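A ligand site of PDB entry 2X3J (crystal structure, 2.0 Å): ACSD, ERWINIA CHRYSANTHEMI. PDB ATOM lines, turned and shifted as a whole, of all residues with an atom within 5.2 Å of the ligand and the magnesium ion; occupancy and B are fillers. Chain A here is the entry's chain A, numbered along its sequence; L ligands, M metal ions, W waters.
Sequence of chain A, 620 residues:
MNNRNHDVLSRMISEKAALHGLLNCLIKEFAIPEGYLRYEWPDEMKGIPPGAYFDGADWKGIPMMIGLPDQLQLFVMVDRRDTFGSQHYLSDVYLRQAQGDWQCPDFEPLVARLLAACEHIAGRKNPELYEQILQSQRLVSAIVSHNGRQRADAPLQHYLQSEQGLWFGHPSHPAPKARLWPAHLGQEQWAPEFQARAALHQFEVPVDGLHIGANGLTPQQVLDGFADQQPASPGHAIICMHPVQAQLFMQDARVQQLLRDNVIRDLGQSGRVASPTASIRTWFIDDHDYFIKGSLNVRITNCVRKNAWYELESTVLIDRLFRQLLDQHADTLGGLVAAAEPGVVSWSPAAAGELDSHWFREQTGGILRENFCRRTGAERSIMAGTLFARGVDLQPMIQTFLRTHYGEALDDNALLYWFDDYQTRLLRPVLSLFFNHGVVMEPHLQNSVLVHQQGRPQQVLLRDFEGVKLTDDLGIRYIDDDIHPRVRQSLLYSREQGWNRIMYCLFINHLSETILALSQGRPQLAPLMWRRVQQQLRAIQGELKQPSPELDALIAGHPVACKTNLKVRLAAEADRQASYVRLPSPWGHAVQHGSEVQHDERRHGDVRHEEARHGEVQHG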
ATOM      1  N   LEU A 166      -3.328  -2.203 -24.663  1.00  0.00           N
ATOM      2  CA  LEU A 166      -4.730  -2.041 -25.031  1.00  0.00           C
ATOM      3  C   LEU A 166      -4.795  -1.890 -26.553  1.00  0.00           C
ATOM      4  O   LEU A 166      -5.123  -0.801 -27.081  1.00  0.00           O
ATOM      5  CB  LEU A 166      -5.395  -0.859 -24.324  1.00  0.00           C
ATOM      6  CG  LEU A 166      -6.933  -0.735 -24.275  1.00  0.00           C
ATOM      7  CD1 LEU A 166      -7.603  -1.799 -23.414  1.00  0.00           C
ATOM      8  CD2 LEU A 166      -7.328   0.640 -23.764  1.00  0.00           C
ATOM      9  N   GLY A 169      -8.237  -0.697 -27.964  1.00  0.00           N
ATOM     10  CA  GLY A 169      -8.810   0.474 -27.323  1.00  0.00           C
ATOM     11  C   GLY A 169     -10.205   0.234 -26.789  1.00  0.00           C
ATOM     12  O   GLY A 169     -10.646  -0.899 -26.646  1.00  0.00           O
ATOM     13  N   HIS A 170     -10.894   1.333 -26.500  1.00  0.00           N
ATOM     14  CA  HIS A 170     -12.308   1.299 -26.126  1.00  0.00           C
ATOM     15  C   HIS A 170     -13.100   0.303 -26.984  1.00  0.00           C
ATOM     16  O   HIS A 170     -13.163   0.423 -28.214  1.00  0.00           O
ATOM     17  CB  HIS A 170     -12.887   2.713 -26.249  1.00  0.00           C
ATOM     18  CG  HIS A 170     -14.134   2.935 -25.453  1.00  0.00           C
ATOM     19  ND1 HIS A 170     -15.201   2.059 -25.454  1.00  0.00           N
ATOM     20  CD2 HIS A 170     -14.497   3.980 -24.667  1.00  0.00           C
ATOM     21  CE1 HIS A 170     -16.173   2.543 -24.697  1.00  0.00           C
ATOM     22  NE2 HIS A 170     -15.780   3.715 -24.217  1.00  0.00           N
ATOM     23  N   PRO A 171     -13.711  -0.700 -26.330  1.00  0.00           N
ATOM     24  CA  PRO A 171     -14.312  -1.775 -27.106  1.00  0.00           C
ATOM     25  C   PRO A 171     -15.664  -1.433 -27.732  1.00  0.00           C
ATOM     26  O   PRO A 171     -16.191  -2.223 -28.523  1.00  0.00           O
ATOM     27  CB  PRO A 171     -14.457  -2.923 -26.090  1.00  0.00           C
ATOM     28  CG  PRO A 171     -14.494  -2.250 -24.741  1.00  0.00           C
ATOM     29  CD  PRO A 171     -13.865  -0.887 -24.871  1.00  0.00           C
ATOM     30  N   PRO A 176     -11.540   3.923 -31.830  1.00  0.00           N
ATOM     31  CA  PRO A 176     -10.828   4.040 -30.546  1.00  0.00           C
ATOM     32  C   PRO A 176      -9.374   4.518 -30.631  1.00  0.00           C
ATOM     33  O   PRO A 176      -8.802   4.931 -29.619  1.00  0.00           O
ATOM     34  CB  PRO A 176     -10.878   2.613 -29.989  1.00  0.00           C
ATOM     35  CG  PRO A 176     -11.031   1.731 -31.213  1.00  0.00           C
ATOM     36  CD  PRO A 176     -11.944   2.534 -32.097  1.00  0.00           C
ATOM     37  N   THR A 277       0.973   6.425 -21.248  1.00  0.00           N
ATOM     38  CA  THR A 277       0.018   5.399 -20.852  1.00  0.00           C
ATOM     39  C   THR A 277      -1.117   5.394 -21.875  1.00  0.00           C
ATOM     40  O   THR A 277      -1.061   6.116 -22.866  1.00  0.00           O
ATOM     41  CB  THR A 277      -0.511   5.668 -19.423  1.00  0.00           C
ATOM     42  OG1 THR A 277      -1.151   6.946 -19.392  1.00  0.00           O
ATOM     43  CG2 THR A 277       0.653   5.699 -18.420  1.00  0.00           C
ATOM     44  N   ALA A 278      -2.147   4.583 -21.624  1.00  0.00           N
ATOM     45  CA  ALA A 278      -3.276   4.443 -22.525  1.00  0.00           C
ATOM     46  C   ALA A 278      -4.033   5.739 -22.761  1.00  0.00           C
ATOM     47  O   ALA A 278      -4.627   5.922 -23.801  1.00  0.00           O
ATOM     48  CB  ALA A 278      -4.213   3.364 -22.035  1.00  0.00           C
ATOM     49  N   SER A 279      -4.014   6.655 -21.797  1.00  0.00           N
ATOM     50  CA  SER A 279      -4.666   7.945 -22.011  1.00  0.00           C
ATOM     51  C   SER A 279      -3.837   8.948 -22.850  1.00  0.00           C
ATOM     52  O   SER A 279      -4.269  10.079 -23.068  1.00  0.00           O
ATOM     53  CB  SER A 279      -5.080   8.559 -20.682  1.00  0.00           C
ATOM     54  OG  SER A 279      -3.947   8.973 -19.947  1.00  0.00           O
ATOM     55  N   ARG A 281      -1.812  11.326 -22.974  1.00  0.00           N
ATOM     56  CA  ARG A 281      -1.215  12.528 -22.384  1.00  0.00           C
ATOM     57  C   ARG A 281      -0.775  12.391 -20.922  1.00  0.00           C
ATOM     58  O   ARG A 281      -0.329  13.370 -20.301  1.00  0.00           O
ATOM     59  CB  ARG A 281      -2.113  13.763 -22.587  1.00  0.00           C
ATOM     60  CG  ARG A 281      -3.605  13.572 -22.341  1.00  0.00           C
ATOM     61  CD  ARG A 281      -3.975  13.288 -20.889  1.00  0.00           C
ATOM     62  NE  ARG A 281      -5.382  13.604 -20.585  1.00  0.00           N
ATOM     63  CZ  ARG A 281      -5.833  14.808 -20.229  1.00  0.00           C
ATOM     64  NH1 ARG A 281      -4.999  15.845 -20.123  1.00  0.00           N
ATOM     65  NH2 ARG A 281      -7.113  14.983 -19.977  1.00  0.00           N
ATOM     66  N   THR A 282      -0.931  11.196 -20.359  1.00  0.00           N
ATOM     67  CA  THR A 282      -0.367  10.864 -19.040  1.00  0.00           C
ATOM     68  C   THR A 282       0.801   9.891 -19.215  1.00  0.00           C
ATOM     69  O   THR A 282       0.660   8.837 -19.876  1.00  0.00           O
ATOM     70  CB  THR A 282      -1.432  10.277 -18.086  1.00  0.00           C
ATOM     71  OG1 THR A 282      -2.521  11.219 -17.964  1.00  0.00           O
ATOM     72  CG2 THR A 282      -0.865  10.029 -16.661  1.00  0.00           C
ATOM     73  N   LYS A 293       0.732  14.107 -15.970  1.00  0.00           N
ATOM     74  CA  LYS A 293      -0.408  14.311 -16.842  1.00  0.00           C
ATOM     75  C   LYS A 293      -0.371  15.747 -17.370  1.00  0.00           C
ATOM     76  O   LYS A 293      -0.325  16.689 -16.595  1.00  0.00           O
ATOM     77  CB  LYS A 293      -1.709  14.022 -16.094  1.00  0.00           C
ATOM     78  CG  LYS A 293      -2.983  14.484 -16.797  1.00  0.00           C
ATOM     79  CD  LYS A 293      -4.208  14.004 -16.039  1.00  0.00           C
ATOM     80  CE  LYS A 293      -5.468  14.329 -16.838  1.00  0.00           C
ATOM     81  NZ  LYS A 293      -6.668  13.768 -16.156  1.00  0.00           N
ATOM     82  N   ILE A 300      -9.143  12.820 -28.801  1.00  0.00           N
ATOM     83  CA  ILE A 300      -8.927  11.398 -28.656  1.00  0.00           C
ATOM     84  C   ILE A 300     -10.215  10.828 -28.098  1.00  0.00           C
ATOM     85  O   ILE A 300     -10.720  11.274 -27.050  1.00  0.00           O
ATOM     86  CB  ILE A 300      -7.756  11.076 -27.684  1.00  0.00           C
ATOM     87  CG1 ILE A 300      -6.446  11.722 -28.184  1.00  0.00           C
ATOM     88  CG2 ILE A 300      -7.612   9.543 -27.511  1.00  0.00           C
ATOM     89  CD1 ILE A 300      -5.419  11.959 -27.103  1.00  0.00           C
ATOM     90  N   THR A 301     -10.737   9.812 -28.800  1.00  0.00           N
ATOM     91  CA  THR A 301     -12.112   9.355 -28.624  1.00  0.00           C
ATOM     92  C   THR A 301     -13.038  10.563 -28.501  1.00  0.00           C
ATOM     93  O   THR A 301     -12.970  11.447 -29.363  1.00  0.00           O
ATOM     94  CB  THR A 301     -12.284   8.242 -27.528  1.00  0.00           C
ATOM     95  OG1 THR A 301     -11.793   8.691 -26.262  1.00  0.00           O
ATOM     96  CG2 THR A 301     -11.563   6.952 -27.946  1.00  0.00           C
ATOM     97  N   ARG A 305      -8.320  16.637 -25.209  1.00  0.00           N
ATOM     98  CA  ARG A 305      -7.670  16.179 -23.974  1.00  0.00           C
ATOM     99  C   ARG A 305      -6.830  17.276 -23.288  1.00  0.00           C
ATOM    100  O   ARG A 305      -5.707  17.045 -22.847  1.00  0.00           O
ATOM    101  CB  ARG A 305      -6.881  14.890 -24.254  1.00  0.00           C
ATOM    102  CG  ARG A 305      -7.706  13.730 -24.806  1.00  0.00           C
ATOM    103  CD  ARG A 305      -8.841  13.336 -23.839  1.00  0.00           C
ATOM    104  NE  ARG A 305      -9.758  12.353 -24.408  1.00  0.00           N
ATOM    105  CZ  ARG A 305     -10.729  11.742 -23.734  1.00  0.00           C
ATOM    106  NH1 ARG A 305     -10.911  12.022 -22.437  1.00  0.00           N
ATOM    107  NH2 ARG A 305     -11.512  10.855 -24.333  1.00  0.00           N
ATOM    108  N   ARG A 369       0.155  12.772 -10.606  1.00  0.00           N
ATOM    109  CA  ARG A 369      -0.638  11.723  -9.993  1.00  0.00           C
ATOM    110  C   ARG A 369       0.333  10.776  -9.298  1.00  0.00           C
ATOM    111  O   ARG A 369       1.351  10.414  -9.867  1.00  0.00           O
ATOM    112  CB  ARG A 369      -1.471  10.970 -11.035  1.00  0.00           C
ATOM    113  CG  ARG A 369      -2.230   9.760 -10.505  1.00  0.00           C
ATOM    114  CD  ARG A 369      -3.080   9.070 -11.587  1.00  0.00           C
ATOM    115  NE  ARG A 369      -4.133   9.968 -12.049  1.00  0.00           N
ATOM    116  CZ  ARG A 369      -4.420  10.238 -13.320  1.00  0.00           C
ATOM    117  NH1 ARG A 369      -3.781   9.607 -14.306  1.00  0.00           N
ATOM    118  NH2 ARG A 369      -5.375  11.127 -13.606  1.00  0.00           N
ATOM    119  N   GLU A 442     -15.859   8.548 -11.978  1.00  0.00           N
ATOM    120  CA  GLU A 442     -16.072   8.075 -13.349  1.00  0.00           C
ATOM    121  C   GLU A 442     -15.387   6.709 -13.503  1.00  0.00           C
ATOM    122  O   GLU A 442     -14.333   6.610 -14.113  1.00  0.00           O
ATOM    123  CB  GLU A 442     -15.565   9.102 -14.361  1.00  0.00           C
ATOM    124  CG  GLU A 442     -16.199   8.925 -15.754  1.00  0.00           C
ATOM    125  CD  GLU A 442     -15.614   9.808 -16.854  1.00  0.00           C
ATOM    126  OE1 GLU A 442     -14.733  10.659 -16.577  1.00  0.00           O
ATOM    127  OE2 GLU A 442     -16.054   9.635 -18.017  1.00  0.00           O
ATOM    128  N   HIS A 444     -14.984   4.091 -15.221  1.00  0.00           N
ATOM    129  CA  HIS A 444     -14.870   3.295 -16.435  1.00  0.00           C
ATOM    130  C   HIS A 444     -13.591   2.468 -16.409  1.00  0.00           C
ATOM    131  O   HIS A 444     -12.782   2.562 -15.457  1.00  0.00           O
ATOM    132  CB  HIS A 444     -15.020   4.145 -17.717  1.00  0.00           C
ATOM    133  CG  HIS A 444     -14.037   5.270 -17.849  1.00  0.00           C
ATOM    134  ND1 HIS A 444     -12.675   5.086 -17.770  1.00  0.00           N
ATOM    135  CD2 HIS A 444     -14.236   6.586 -18.087  1.00  0.00           C
ATOM    136  CE1 HIS A 444     -12.068   6.252 -17.963  1.00  0.00           C
ATOM    137  NE2 HIS A 444     -12.995   7.174 -18.161  1.00  0.00           N
ATOM    138  N   LEU A 445     -13.400   1.647 -17.433  1.00  0.00           N
ATOM    139  CA  LEU A 445     -12.322   0.654 -17.428  1.00  0.00           C
ATOM    140  C   LEU A 445     -10.914   1.251 -17.333  1.00  0.00           C
ATOM    141  O   LEU A 445     -10.021   0.661 -16.681  1.00  0.00           O
ATOM    142  CB  LEU A 445     -12.439  -0.267 -18.645  1.00  0.00           C
ATOM    143  CG  LEU A 445     -13.462  -1.399 -18.547  1.00  0.00           C
ATOM    144  CD1 LEU A 445     -13.630  -2.021 -19.933  1.00  0.00           C
ATOM    145  CD2 LEU A 445     -13.031  -2.459 -17.519  1.00  0.00           C
ATOM    146  N   GLN A 446     -10.737   2.416 -17.946  1.00  0.00           N
ATOM    147  CA  GLN A 446      -9.445   3.098 -17.950  1.00  0.00           C
ATOM    148  C   GLN A 446      -9.144   3.883 -16.682  1.00  0.00           C
ATOM    149  O   GLN A 446      -7.985   4.219 -16.423  1.00  0.00           O
ATOM    150  CB  GLN A 446      -9.283   3.974 -19.195  1.00  0.00           C
ATOM    151  CG  GLN A 446      -7.886   4.620 -19.362  1.00  0.00           C
ATOM    152  CD  GLN A 446      -7.755   5.941 -18.597  1.00  0.00           C
ATOM    153  OE1 GLN A 446      -8.745   6.526 -18.160  1.00  0.00           O
ATOM    154  NE2 GLN A 446      -6.518   6.390 -18.384  1.00  0.00           N
ATOM    155  N   ASN A 447     -10.172   4.195 -15.900  1.00  0.00           N
ATOM    156  CA  ASN A 447      -9.981   4.856 -14.618  1.00  0.00           C
ATOM    157  C   ASN A 447      -9.854   3.870 -13.465  1.00  0.00           C
ATOM    158  O   ASN A 447      -9.911   4.265 -12.305  1.00  0.00           O
ATOM    159  CB  ASN A 447     -11.136   5.826 -14.365  1.00  0.00           C
ATOM    160  CG  ASN A 447     -10.971   7.131 -15.113  1.00  0.00           C
ATOM    161  OD1 ASN A 447      -9.869   7.457 -15.591  1.00  0.00           O
ATOM    162  ND2 ASN A 447     -12.054   7.895 -15.221  1.00  0.00           N
ATOM    163  N   ARG A 463      -8.933   6.199 -10.195  1.00  0.00           N
ATOM    164  CA  ARG A 463      -8.123   7.358 -10.525  1.00  0.00           C
ATOM    165  C   ARG A 463      -8.870   8.374 -11.384  1.00  0.00           C
ATOM    166  O   ARG A 463      -9.972   8.077 -11.884  1.00  0.00           O
ATOM    167  CB  ARG A 463      -6.828   6.935 -11.225  1.00  0.00           C
ATOM    168  CG  ARG A 463      -7.038   6.267 -12.578  1.00  0.00           C
ATOM    169  CD  ARG A 463      -5.776   6.240 -13.419  1.00  0.00           C
ATOM    170  NE  ARG A 463      -5.924   5.292 -14.523  1.00  0.00           N
ATOM    171  CZ  ARG A 463      -4.959   4.524 -14.990  1.00  0.00           C
ATOM    172  NH1 ARG A 463      -3.737   4.556 -14.432  1.00  0.00           N
ATOM    173  NH2 ARG A 463      -5.204   3.689 -15.983  1.00  0.00           N
ATOM    174  N   ASP A 464      -8.251   9.537 -11.541  1.00  0.00           N
ATOM    175  CA  ASP A 464      -8.681  10.627 -12.428  1.00  0.00           C
ATOM    176  C   ASP A 464      -9.674  11.564 -11.748  1.00  0.00           C
ATOM    177  O   ASP A 464     -10.889  11.365 -11.796  1.00  0.00           O
ATOM    178  CB  ASP A 464      -9.166  10.075 -13.779  1.00  0.00           C
ATOM    179  CG  ASP A 464      -9.285  11.146 -14.844  1.00  0.00           C
ATOM    180  OD1 ASP A 464      -9.551  10.766 -16.010  1.00  0.00           O
ATOM    181  OD2 ASP A 464      -9.119  12.347 -14.538  1.00  0.00           O
ATOM    182  N   GLU A 466     -10.157  14.680 -12.401  1.00  0.00           N
ATOM    183  CA  GLU A 466     -10.563  15.786 -13.257  1.00  0.00           C
ATOM    184  C   GLU A 466     -11.943  15.513 -13.788  1.00  0.00           C
ATOM    185  O   GLU A 466     -12.631  16.435 -14.250  1.00  0.00           O
ATOM    186  CB  GLU A 466      -9.552  15.961 -14.385  1.00  0.00           C
ATOM    187  CG  GLU A 466      -8.129  16.288 -13.875  1.00  0.00           C
ATOM    188  CD  GLU A 466      -7.405  15.054 -13.346  1.00  0.00           C
ATOM    189  OE1 GLU A 466      -7.871  14.466 -12.373  1.00  0.00           O
ATOM    190  OE2 GLU A 466      -6.381  14.649 -13.887  1.00  0.00           O
ATOM    191  N   ASN A 509     -20.159   0.048 -19.240  1.00  0.00           N
ATOM    192  CA  ASN A 509     -18.757   0.199 -19.615  1.00  0.00           C
ATOM    193  C   ASN A 509     -17.860  -0.858 -18.977  1.00  0.00           C
ATOM    194  O   ASN A 509     -16.998  -1.452 -19.645  1.00  0.00           O
ATOM    195  CB  ASN A 509     -18.279   1.623 -19.256  1.00  0.00           C
ATOM    196  CG  ASN A 509     -16.822   1.900 -19.607  1.00  0.00           C
ATOM    197  OD1 ASN A 509     -15.913   1.384 -18.963  1.00  0.00           O
ATOM    198  ND2 ASN A 509     -16.593   2.732 -20.615  1.00  0.00           N
HETATM  199  P1  LIG L   1      -5.931   9.918 -16.971  1.00  0.00           P
HETATM  200  O1  LIG L   1      -6.846   8.712 -16.764  1.00  0.00           O
HETATM  201  O2  LIG L   1      -4.454   9.552 -17.111  1.00  0.00           O
HETATM  202  O3  LIG L   1      -6.207  11.131 -16.116  1.00  0.00           O
HETATM  203  P2  LIG L   1      -7.654  11.163 -18.984  1.00  0.00           P
HETATM  204  O4  LIG L   1      -8.223  12.168 -18.005  1.00  0.00           O
HETATM  205  O5  LIG L   1      -7.432  11.617 -20.421  1.00  0.00           O
HETATM  206  O6  LIG L   1      -6.259  10.513 -18.446  1.00  0.00           O
HETATM  207  P3  LIG L   1     -10.232   9.940 -19.229  1.00  0.00           P
HETATM  208  O7  LIG L   1     -10.849   9.037 -18.174  1.00  0.00           O
HETATM  209  O8  LIG L   1     -10.672  11.391 -19.336  1.00  0.00           O
HETATM  210  O9  LIG L   1      -8.618   9.858 -19.091  1.00  0.00           O
HETATM  211  O10 LIG L   1     -10.499   9.266 -20.685  1.00  0.00           O
HETATM  212  C1  LIG L   1     -10.197   7.877 -20.857  1.00  0.00           C
HETATM  213  C2  LIG L   1      -9.096   7.647 -21.901  1.00  0.00           C
HETATM  214  O11 LIG L   1      -8.861   6.232 -21.949  1.00  0.00           O
HETATM  215  C3  LIG L   1      -9.529   8.014 -23.311  1.00  0.00           C
HETATM  216  O12 LIG L   1      -8.374   8.399 -24.061  1.00  0.00           O
HETATM  217  C4  LIG L   1     -10.126   6.728 -23.880  1.00  0.00           C
HETATM  218  O13 LIG L   1      -9.973   6.605 -25.304  1.00  0.00           O
HETATM  219  C5  LIG L   1      -9.324   5.643 -23.192  1.00  0.00           C
HETATM  220  N1  LIG L   1     -10.104   4.390 -22.980  1.00  0.00           N
HETATM  221  C6  LIG L   1      -9.689   3.158 -23.340  1.00  0.00           C
HETATM  222  N2  LIG L   1     -10.613   2.227 -23.018  1.00  0.00           N
HETATM  223  C7  LIG L   1     -11.642   2.857 -22.430  1.00  0.00           C
HETATM  224  C8  LIG L   1     -12.947   2.447 -21.857  1.00  0.00           C
HETATM  225  N3  LIG L   1     -13.352   1.146 -21.860  1.00  0.00           N
HETATM  226  N4  LIG L   1     -13.719   3.423 -21.345  1.00  0.00           N
HETATM  227  C9  LIG L   1     -13.360   4.713 -21.358  1.00  0.00           C
HETATM  228  N5  LIG L   1     -12.194   5.154 -21.865  1.00  0.00           N
HETATM  229  C10 LIG L   1     -11.312   4.272 -22.404  1.00  0.00           C
HETATM  230 MG    MG M   1      -8.953   8.602 -17.040  1.00  0.00          MG
HETATM  231  O   HOH W   1      -3.086   7.112 -16.940  1.00  0.00           O
HETATM  232  O   HOH W   2      -6.723   6.354 -25.547  1.00  0.00           O
HETATM  233  O   HOH W   3      -7.206  10.683 -23.062  1.00  0.00           O
HETATM  234  O   HOH W   4     -11.177  -0.549 -22.357  1.00  0.00           O
HETATM  235  O   HOH W   5      -9.039  14.985 -17.469  1.00  0.00           O
HETATM  236  O   HOH W   6      -9.599   4.006 -27.049  1.00  0.00           O
HETATM  237  O   HOH W   7     -16.331  -0.424 -22.137  1.00  0.00           O
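The side-chain hydroxyl of Thr 301 sits at hydrogen-bond distance from the guanidinium group of Arg 305 (2.9 Å).
The backbone carbonyl oxygen (O) of Thr 282 is in hydrogen-bond range of the side-chain hydroxyl (OG1) of Thr 277 (2.7 Å).
The backbone carbonyl oxygen (O) of Arg 305 is in hydrogen-bond range of the guanidinium group (NH1) of Arg 281 (3.1 Å).
The side-chain amide nitrogen of Asn 447 sits at hydrogen-bond distance from the backbone carbonyl oxygen of Glu 442, at 2.8 Å.
The guanidinium group of Arg 369 lies within salt-bridge range of the side-chain carboxylate of Glu 466, at 3.7 Å.
The backbone carbonyl oxygen (O) of Gln 446 is in hydrogen-bond range of the guanidinium group (NH2) of Arg 463, 2.9 Å away.
The backbone carbonyl oxygen of Ile 300 sits at hydrogen-bond distance from the guanidinium group of Arg 305 (2.9 Å).
N of Leu 445 is in hydrogen-bond range of OD1 of Asn 509, 3.0 Å away.
OG1 of Thr 282 lies within hydrogen-bond range of O2 of the ligand (2.7 Å).
NE of Arg 281 lies within salt-bridge range of O5 of the ligand, at 2.9 Å.
An oxygen (O7) of the ligand sits close to a ring nitrogen (NE2) of His 444 (2.8 Å).
O2 of the ligand sits at hydrogen-bond distance from OG of Ser 279 (2.9 Å).
NZ of Lys 293 is in salt-bridge range of O3 of the ligand (2.7 Å).
An oxygen (O3) of the ligand is in salt-bridge range of the guanidinium group (NH2) of Arg 369 (2.6 Å).
OG1 of Thr 301 is in hydrogen-bond range of O13 of the ligand (2.9 Å).
N4 of the ligand is in hydrogen-bond range of ND2 of Asn 509, at 3.0 Å.
NH1 of Arg 305 is in salt-bridge range of O8 of the ligand, at 3.2 Å.
Merely in contact with the ligand: Leu 166 (3.5 Å), His 170 (3.5 Å), Pro 171 (3.7 Å), Ile 300 (3.7 Å) and Leu 445 (3.6 Å).
17 residues have an atom within 4 Å of the ligand: Leu 166, His 170, Pro 171, Ser 279, Arg 281, Thr 282, Lys 293, Ile 300, Thr 301, Arg 305, Arg 369, His 444, Leu 445, Gln 446, Asn 447, Asp 464 and Asn 509.
The nearest printed residue that does not touch the ligand is Glu 466 (4.2 Å).
Water W3 lies within hydrogen-bond range of O12 of the ligand (2.8 Å), O of Ser 279 (3.0 Å) and NE of Arg 305 (3.3 Å).
Water W1 lies within hydrogen-bond range of O2 of the ligand and OG1 of Thr 277.
Water W5 lies within hydrogen-bond range of the side-chain amino group (NZ) of Lys 293, an oxygen (O4) of the ligand and the guanidinium group (NH2) of Arg 281.
Water W2 lies within hydrogen-bond range of O of Ala 278 (2.8 Å) and O12 of the ligand (3.0 Å).
Water W6 lies within hydrogen-bond range of the backbone carbonyl oxygen (O) of Pro 176 (2.8 Å), the backbone NH (N) of His 170 (3.0 Å) and an oxygen (O13) of the ligand (3.2 Å).
Water W7 lies within hydrogen-bond range of the backbone carbonyl oxygen of Asn 509 (2.8 Å) and a nitrogen (N3) of the ligand (3.4 Å).
OD1 of Asn 447 binds the magnesium ion (2.1 Å).
O1 of the ligand binds the magnesium ion (2.1 Å).
O7 of the ligand is bound to the magnesium ion, 2.3 Å away.
The magnesium ion is bound by OE1 of Gln 446, at 2.4 Å.
An oxygen (O9) of the ligand binds the magnesium ion (2.4 Å).
OD1 of Asp 464 binds the magnesium ion, at 2.5 Å.
Within 4 Å of the magnesium ion: Gln 446, Asn 447 and Asp 464.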
